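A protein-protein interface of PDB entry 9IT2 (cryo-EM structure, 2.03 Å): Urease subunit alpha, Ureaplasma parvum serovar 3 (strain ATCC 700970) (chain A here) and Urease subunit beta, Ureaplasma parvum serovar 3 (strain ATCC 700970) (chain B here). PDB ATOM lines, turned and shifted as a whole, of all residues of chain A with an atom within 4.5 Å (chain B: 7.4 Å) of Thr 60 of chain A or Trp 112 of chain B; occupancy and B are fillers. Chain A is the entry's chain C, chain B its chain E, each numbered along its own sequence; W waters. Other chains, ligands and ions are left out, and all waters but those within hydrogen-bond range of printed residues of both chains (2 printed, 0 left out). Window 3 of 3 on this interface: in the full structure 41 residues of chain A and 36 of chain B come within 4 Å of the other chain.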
ATOM      1  N   GLY A  54      12.719   5.019  11.010  1.00  0.00           N
ATOM      2  CA  GLY A  54      13.846   5.864  10.695  1.00  0.00           C
ATOM      3  C   GLY A  54      13.877   7.204  11.397  1.00  0.00           C
ATOM      4  O   GLY A  54      14.919   7.870  11.370  1.00  0.00           O
ATOM      5  N   ASN A  58      13.967   2.925  15.474  1.00  0.00           N
ATOM      6  CA  ASN A  58      15.112   2.394  14.752  1.00  0.00           C
ATOM      7  C   ASN A  58      14.661   1.330  13.756  1.00  0.00           C
ATOM      8  O   ASN A  58      13.733   0.559  14.012  1.00  0.00           O
ATOM      9  CB  ASN A  58      16.131   1.810  15.729  1.00  0.00           C
ATOM     10  CG  ASN A  58      17.342   1.225  15.032  1.00  0.00           C
ATOM     11  OD1 ASN A  58      17.362   0.046  14.682  1.00  0.00           O
ATOM     12  ND2 ASN A  58      18.362   2.048  14.829  1.00  0.00           N
ATOM     13  N   SER A  59      15.331   1.295  12.605  1.00  0.00           N
ATOM     14  CA  SER A  59      14.927   0.432  11.507  1.00  0.00           C
ATOM     15  C   SER A  59      15.959  -0.625  11.135  1.00  0.00           C
ATOM     16  O   SER A  59      15.707  -1.410  10.214  1.00  0.00           O
ATOM     17  CB  SER A  59      14.597   1.277  10.269  1.00  0.00           C
ATOM     18  OG  SER A  59      15.777   1.750   9.646  1.00  0.00           O
ATOM     19  N   THR A  60      17.102  -0.674  11.813  1.00  0.00           N
ATOM     20  CA  THR A  60      18.174  -1.596  11.453  1.00  0.00           C
ATOM     21  C   THR A  60      18.378  -2.725  12.450  1.00  0.00           C
ATOM     22  O   THR A  60      18.624  -3.860  12.039  1.00  0.00           O
ATOM     23  CB  THR A  60      19.497  -0.836  11.293  1.00  0.00           C
ATOM     24  OG1 THR A  60      19.889  -0.279  12.554  1.00  0.00           O
ATOM     25  CG2 THR A  60      19.346   0.277  10.278  1.00  0.00           C
ATOM     26  N   MET A  61      18.284  -2.450  13.747  1.00  0.00           N
ATOM     27  CA  MET A  61      18.620  -3.447  14.752  1.00  0.00           C
ATOM     28  C   MET A  61      17.531  -4.502  14.869  1.00  0.00           C
ATOM     29  O   MET A  61      16.336  -4.198  14.816  1.00  0.00           O
ATOM     30  CB  MET A  61      18.849  -2.786  16.111  1.00  0.00           C
ATOM     31  CG  MET A  61      20.051  -1.863  16.147  1.00  0.00           C
ATOM     32  SD  MET A  61      20.076  -0.848  17.629  1.00  0.00           S
ATOM     33  CE  MET A  61      20.480  -2.094  18.849  1.00  0.00           C
ATOM     34  N   LYS A  62      17.955  -5.752  15.026  1.00  0.00           N
ATOM     35  CA  LYS A  62      17.034  -6.846  15.276  1.00  0.00           C
ATOM     36  C   LYS A  62      16.651  -6.879  16.755  1.00  0.00           C
ATOM     37  O   LYS A  62      17.203  -6.152  17.585  1.00  0.00           O
ATOM     38  CB  LYS A  62      17.653  -8.173  14.837  1.00  0.00           C
ATOM     39  CG  LYS A  62      17.703  -8.351  13.326  1.00  0.00           C
ATOM     40  CD  LYS A  62      17.792  -9.816  12.933  1.00  0.00           C
ATOM     41  CE  LYS A  62      19.193 -10.358  13.150  1.00  0.00           C
ATOM     42  NZ  LYS A  62      20.203  -9.607  12.356  1.00  0.00           N
ATOM     43  N   ASP A  65      19.521  -7.506  18.953  1.00  0.00           N
ATOM     44  CA  ASP A  65      20.691  -6.666  18.750  1.00  0.00           C
ATOM     45  C   ASP A  65      20.875  -5.698  19.916  1.00  0.00           C
ATOM     46  O   ASP A  65      19.940  -5.387  20.657  1.00  0.00           O
ATOM     47  CB  ASP A  65      20.576  -5.888  17.439  1.00  0.00           C
ATOM     48  CG  ASP A  65      20.834  -6.755  16.222  1.00  0.00           C
ATOM     49  OD1 ASP A  65      21.343  -7.882  16.391  1.00  0.00           O
ATOM     50  OD2 ASP A  65      20.527  -6.309  15.097  1.00  0.00           O
ATOM     51  N   HIS A 110      20.047   6.608  16.452  1.00  0.00           N
ATOM     52  CA  HIS A 110      20.594   7.144  15.211  1.00  0.00           C
ATOM     53  C   HIS A 110      20.323   8.637  15.070  1.00  0.00           C
ATOM     54  O   HIS A 110      21.120   9.354  14.453  1.00  0.00           O
ATOM     55  CB  HIS A 110      20.018   6.383  14.018  1.00  0.00           C
ATOM     56  CG  HIS A 110      20.609   5.021  13.827  1.00  0.00           C
ATOM     57  ND1 HIS A 110      20.077   4.094  12.956  1.00  0.00           N
ATOM     58  CD2 HIS A 110      21.687   4.429  14.392  1.00  0.00           C
ATOM     59  CE1 HIS A 110      20.801   2.991  12.993  1.00  0.00           C
ATOM     60  NE2 HIS A 110      21.786   3.168  13.856  1.00  0.00           N
ATOM     61  N   HIS B  53      12.996  13.248   8.185  1.00  0.00           N
ATOM     62  CA  HIS B  53      14.172  13.786   7.513  1.00  0.00           C
ATOM     63  C   HIS B  53      13.733  14.681   6.362  1.00  0.00           C
ATOM     64  O   HIS B  53      13.221  14.194   5.349  1.00  0.00           O
ATOM     65  CB  HIS B  53      15.067  12.648   7.017  1.00  0.00           C
ATOM     66  CG  HIS B  53      16.379  13.104   6.458  1.00  0.00           C
ATOM     67  ND1 HIS B  53      17.076  12.382   5.515  1.00  0.00           N
ATOM     68  CD2 HIS B  53      17.122  14.208   6.710  1.00  0.00           C
ATOM     69  CE1 HIS B  53      18.192  13.018   5.210  1.00  0.00           C
ATOM     70  NE2 HIS B  53      18.244  14.130   5.920  1.00  0.00           N
ATOM     71  N   GLU B  56      14.071  14.178   2.542  1.00  0.00           N
ATOM     72  CA  GLU B  56      13.371  13.089   1.869  1.00  0.00           C
ATOM     73  C   GLU B  56      11.862  13.308   1.801  1.00  0.00           C
ATOM     74  O   GLU B  56      11.111  12.351   1.589  1.00  0.00           O
ATOM     75  CB  GLU B  56      13.678  11.759   2.562  1.00  0.00           C
ATOM     76  CG  GLU B  56      15.143  11.580   2.937  1.00  0.00           C
ATOM     77  CD  GLU B  56      15.480  10.154   3.323  1.00  0.00           C
ATOM     78  OE1 GLU B  56      15.017   9.223   2.632  1.00  0.00           O
ATOM     79  OE2 GLU B  56      16.210   9.962   4.319  1.00  0.00           O
ATOM     80  N   THR B 108      24.107   9.362  16.486  1.00  0.00           N
ATOM     81  CA  THR B 108      25.143   8.942  15.554  1.00  0.00           C
ATOM     82  C   THR B 108      24.957   9.546  14.169  1.00  0.00           C
ATOM     83  O   THR B 108      25.812   9.340  13.301  1.00  0.00           O
ATOM     84  CB  THR B 108      25.181   7.414  15.452  1.00  0.00           C
ATOM     85  OG1 THR B 108      23.880   6.922  15.111  1.00  0.00           O
ATOM     86  CG2 THR B 108      25.618   6.803  16.774  1.00  0.00           C
ATOM     87  N   ARG B 109      23.862  10.278  13.954  1.00  0.00           N
ATOM     88  CA  ARG B 109      23.590  10.980  12.700  1.00  0.00           C
ATOM     89  C   ARG B 109      23.593  10.019  11.513  1.00  0.00           C
ATOM     90  O   ARG B 109      24.320  10.199  10.534  1.00  0.00           O
ATOM     91  CB  ARG B 109      24.577  12.132  12.488  1.00  0.00           C
ATOM     92  CG  ARG B 109      24.080  13.466  13.030  1.00  0.00           C
ATOM     93  CD  ARG B 109      25.037  14.606  12.714  1.00  0.00           C
ATOM     94  NE  ARG B 109      24.932  15.043  11.327  1.00  0.00           N
ATOM     95  CZ  ARG B 109      23.978  15.835  10.860  1.00  0.00           C
ATOM     96  NH1 ARG B 109      23.021  16.303  11.644  1.00  0.00           N
ATOM     97  NH2 ARG B 109      23.981  16.164   9.571  1.00  0.00           N
ATOM     98  N   GLU B 110      22.769   8.981  11.614  1.00  0.00           N
ATOM     99  CA  GLU B 110      22.514   8.059  10.520  1.00  0.00           C
ATOM    100  C   GLU B 110      21.017   7.998  10.263  1.00  0.00           C
ATOM    101  O   GLU B 110      20.220   7.946  11.205  1.00  0.00           O
ATOM    102  CB  GLU B 110      23.044   6.651  10.822  1.00  0.00           C
ATOM    103  CG  GLU B 110      24.322   6.611  11.635  1.00  0.00           C
ATOM    104  CD  GLU B 110      24.655   5.212  12.113  1.00  0.00           C
ATOM    105  OE1 GLU B 110      24.866   4.328  11.259  1.00  0.00           O
ATOM    106  OE2 GLU B 110      24.701   4.995  13.342  1.00  0.00           O
ATOM    107  N   VAL B 111      20.637   8.009   8.990  1.00  0.00           N
ATOM    108  CA  VAL B 111      19.241   7.901   8.587  1.00  0.00           C
ATOM    109  C   VAL B 111      19.086   6.610   7.801  1.00  0.00           C
ATOM    110  O   VAL B 111      19.737   6.423   6.766  1.00  0.00           O
ATOM    111  CB  VAL B 111      18.787   9.110   7.755  1.00  0.00           C
ATOM    112  CG1 VAL B 111      17.367   8.902   7.258  1.00  0.00           C
ATOM    113  CG2 VAL B 111      18.888  10.385   8.576  1.00  0.00           C
ATOM    114  N   TRP B 112      18.229   5.720   8.294  1.00  0.00           N
ATOM    115  CA  TRP B 112      17.942   4.448   7.649  1.00  0.00           C
ATOM    116  C   TRP B 112      16.443   4.342   7.422  1.00  0.00           C
ATOM    117  O   TRP B 112      15.655   4.558   8.349  1.00  0.00           O
ATOM    118  CB  TRP B 112      18.436   3.274   8.496  1.00  0.00           C
ATOM    119  CG  TRP B 112      19.927   3.190   8.608  1.00  0.00           C
ATOM    120  CD1 TRP B 112      20.718   3.831   9.516  1.00  0.00           C
ATOM    121  CD2 TRP B 112      20.805   2.403   7.795  1.00  0.00           C
ATOM    122  NE1 TRP B 112      22.036   3.501   9.311  1.00  0.00           N
ATOM    123  CE2 TRP B 112      22.116   2.625   8.261  1.00  0.00           C
ATOM    124  CE3 TRP B 112      20.611   1.538   6.715  1.00  0.00           C
ATOM    125  CZ2 TRP B 112      23.226   2.010   7.686  1.00  0.00           C
ATOM    126  CZ3 TRP B 112      21.715   0.929   6.145  1.00  0.00           C
ATOM    127  CH2 TRP B 112      23.005   1.171   6.630  1.00  0.00           C
ATOM    128  N   GLY B 113      16.055   4.012   6.200  1.00  0.00           N
ATOM    129  CA  GLY B 113      14.647   3.937   5.853  1.00  0.00           C
ATOM    130  C   GLY B 113      14.164   5.239   5.248  1.00  0.00           C
ATOM    131  O   GLY B 113      14.799   5.781   4.342  1.00  0.00           O
ATOM    132  N   VAL B 114      13.047   5.751   5.771  1.00  0.00           N
ATOM    133  CA  VAL B 114      12.363   6.915   5.216  1.00  0.00           C
ATOM    134  C   VAL B 114      12.122   6.656   3.733  1.00  0.00           C
ATOM    135  O   VAL B 114      11.394   5.725   3.370  1.00  0.00           O
ATOM    136  CB  VAL B 114      13.157   8.216   5.455  1.00  0.00           C
ATOM    137  CG1 VAL B 114      12.269   9.432   5.248  1.00  0.00           C
ATOM    138  CG2 VAL B 114      13.740   8.232   6.861  1.00  0.00           C
ATOM    139  N   ASN B 115      12.750   7.444   2.864  1.00  0.00           N
ATOM    140  CA  ASN B 115      12.615   7.259   1.427  1.00  0.00           C
ATOM    141  C   ASN B 115      13.800   6.520   0.819  1.00  0.00           C
ATOM    142  O   ASN B 115      13.902   6.437  -0.408  1.00  0.00           O
ATOM    143  CB  ASN B 115      12.424   8.609   0.734  1.00  0.00           C
ATOM    144  CG  ASN B 115      10.968   8.917   0.452  1.00  0.00           C
ATOM    145  OD1 ASN B 115      10.164   8.014   0.223  1.00  0.00           O
ATOM    146  ND2 ASN B 115      10.620  10.198   0.468  1.00  0.00           N
ATOM    147  N   GLY B 116      14.693   5.982   1.647  1.00  0.00           N
ATOM    148  CA  GLY B 116      15.844   5.267   1.137  1.00  0.00           C
ATOM    149  C   GLY B 116      16.887   6.141   0.484  1.00  0.00           C
ATOM    150  O   GLY B 116      17.774   5.625  -0.200  1.00  0.00           O
ATOM    151  N   VAL B 118      19.206   8.136   1.938  1.00  0.00           N
ATOM    152  CA  VAL B 118      20.486   8.078   2.641  1.00  0.00           C
ATOM    153  C   VAL B 118      20.859   6.638   2.986  1.00  0.00           C
ATOM    154  O   VAL B 118      21.857   6.111   2.488  1.00  0.00           O
ATOM    155  CB  VAL B 118      20.470   8.970   3.902  1.00  0.00           C
ATOM    156  CG1 VAL B 118      21.844   8.995   4.555  1.00  0.00           C
ATOM    157  CG2 VAL B 118      20.011  10.378   3.551  1.00  0.00           C
ATOM    158  N   ASN B 119      20.056   5.979   3.823  1.00  0.00           N
ATOM    159  CA  ASN B 119      20.290   4.600   4.260  1.00  0.00           C
ATOM    160  C   ASN B 119      21.722   4.409   4.760  1.00  0.00           C
ATOM    161  O   ASN B 119      22.441   3.499   4.343  1.00  0.00           O
ATOM    162  CB  ASN B 119      19.957   3.607   3.147  1.00  0.00           C
ATOM    163  CG  ASN B 119      18.494   3.208   3.147  1.00  0.00           C
ATOM    164  OD1 ASN B 119      17.718   3.662   3.987  1.00  0.00           O
ATOM    165  ND2 ASN B 119      18.110   2.355   2.206  1.00  0.00           N
ATOM    166  N   GLY B 120      22.135   5.288   5.664  1.00  0.00           N
ATOM    167  CA  GLY B 120      23.477   5.220   6.210  1.00  0.00           C
ATOM    168  C   GLY B 120      23.829   6.514   6.923  1.00  0.00           C
ATOM    169  O   GLY B 120      22.959   7.327   7.229  1.00  0.00           O
ATOM    170  N   LYS B 121      25.123   6.672   7.181  1.00  0.00           N
ATOM    171  CA  LYS B 121      25.615   7.867   7.850  1.00  0.00           C
ATOM    172  C   LYS B 121      25.472   9.088   6.952  1.00  0.00           C
ATOM    173  O   LYS B 121      25.740   9.031   5.748  1.00  0.00           O
ATOM    174  CB  LYS B 121      27.077   7.686   8.255  1.00  0.00           C
ATOM    175  CG  LYS B 121      27.337   6.480   9.140  1.00  0.00           C
ATOM    176  CD  LYS B 121      28.652   6.623   9.889  1.00  0.00           C
ATOM    177  CE  LYS B 121      28.713   7.936  10.652  1.00  0.00           C
ATOM    178  NZ  LYS B 121      28.645   7.733  12.126  1.00  0.00           N
HETATM  179  O   HOH W   1      13.970  10.853  10.224  1.00  0.00           O
HETATM  180  O   HOH W   2      17.361   6.867  11.179  1.00  0.00           O
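The side-chain carboxylate of Glu 110 of chain B is in hydrogen-bond range of the side-chain hydroxyl of Thr 108 of chain B (2.7 Å). The backbone carbonyl oxygen (O) of Thr 108 of chain B sits at hydrogen-bond distance from the side-chain amino group (NZ) of Lys 121 of chain B, at 3.5 Å. The side-chain amide oxygen of Asn 58 of chain A sits at hydrogen-bond distance from the backbone NH of Thr 60 of chain A (3.0 Å). The side-chain amide nitrogen (ND2) of Asn 58 of chain A sits close to a ring nitrogen (ND1) of His 110 of chain A, 3.3 Å away.
The backbone NH (N) of Arg 109 of chain B lies within hydrogen-bond range of the backbone carbonyl oxygen (O) of His 110 of chain A. The backbone NH of Glu 110 of chain B sits at hydrogen-bond distance from the backbone carbonyl oxygen of His 110 of chain A. The backbone carbonyl oxygen (O) of Trp 112 of chain B lies within hydrogen-bond range of the side-chain hydroxyl (OG) of Ser 59 of chain A, 3.1 Å away.
Among the printed residues, pairs that only touch across the chains: Gly 54 of chain A with Trp 112 of chain B (3.2 Å), His 110 of chain A with Thr 108 of chain B (3.3 Å), Thr 60 of chain A with Trp 112 of chain B (3.4 Å) and His 110 of chain A with Trp 112 of chain B (3.5 Å).
Water W2 lies within hydrogen-bond range of O of Gly 54 of chain A (2.6 Å), O of Glu 110 of chain B (3.1 Å) and N of Trp 112 of chain B (3.2 Å). Water W1 lies within hydrogen-bond range of the backbone NH (N) of His 53 of chain B (3.3 Å) and the backbone carbonyl oxygen (O) of Gly 54 of chain A (3.3 Å).
Of the 15 printed residues of chain B, 4 touch a printed residue of chain A. Hydrophobic or aromatic side chains of chain B that line the printed part of chain A: Trp 112. Hydrophobic or aromatic side chains of chain A that line the printed part of chain B: His 110. Along chain A the printed residues that touch a printed residue of chain B span positions 54 to 110. Among the printed residues, 7 pairs touch across the chains. Among the printed residues, no Asp or Glu carboxylate lies within 4 Å of a Lys or Arg side-chain nitrogen of the other chain.
Thr 60 of chain A touches just one residue of chain B: Trp 112. Trp 112 of chain B touches just these residues of chain A: Gly 54 (3.2 Å), Ser 59 (3.1 Å), Thr 60 (3.4 Å) and His 110 (3.5 Å). Of the printed residues of chain A, Arg 109 of chain B touches His 110. Of the printed residues of chain B, His 110 of chain A touches Thr 108 (3.3 Å), Arg 109 (2.9 Å), Glu 110 (3.2 Å) and Trp 112 (3.5 Å). Asn 115 of chain B touches none of the printed residues of chain A. The nearest residue of chain B that does not touch Thr 60 of chain A is Gly 113 of chain B (6.4 Å). The nearest printed residue of chain B that does not touch His 110 of chain A is Val 111 of chain B (5.3 Å).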
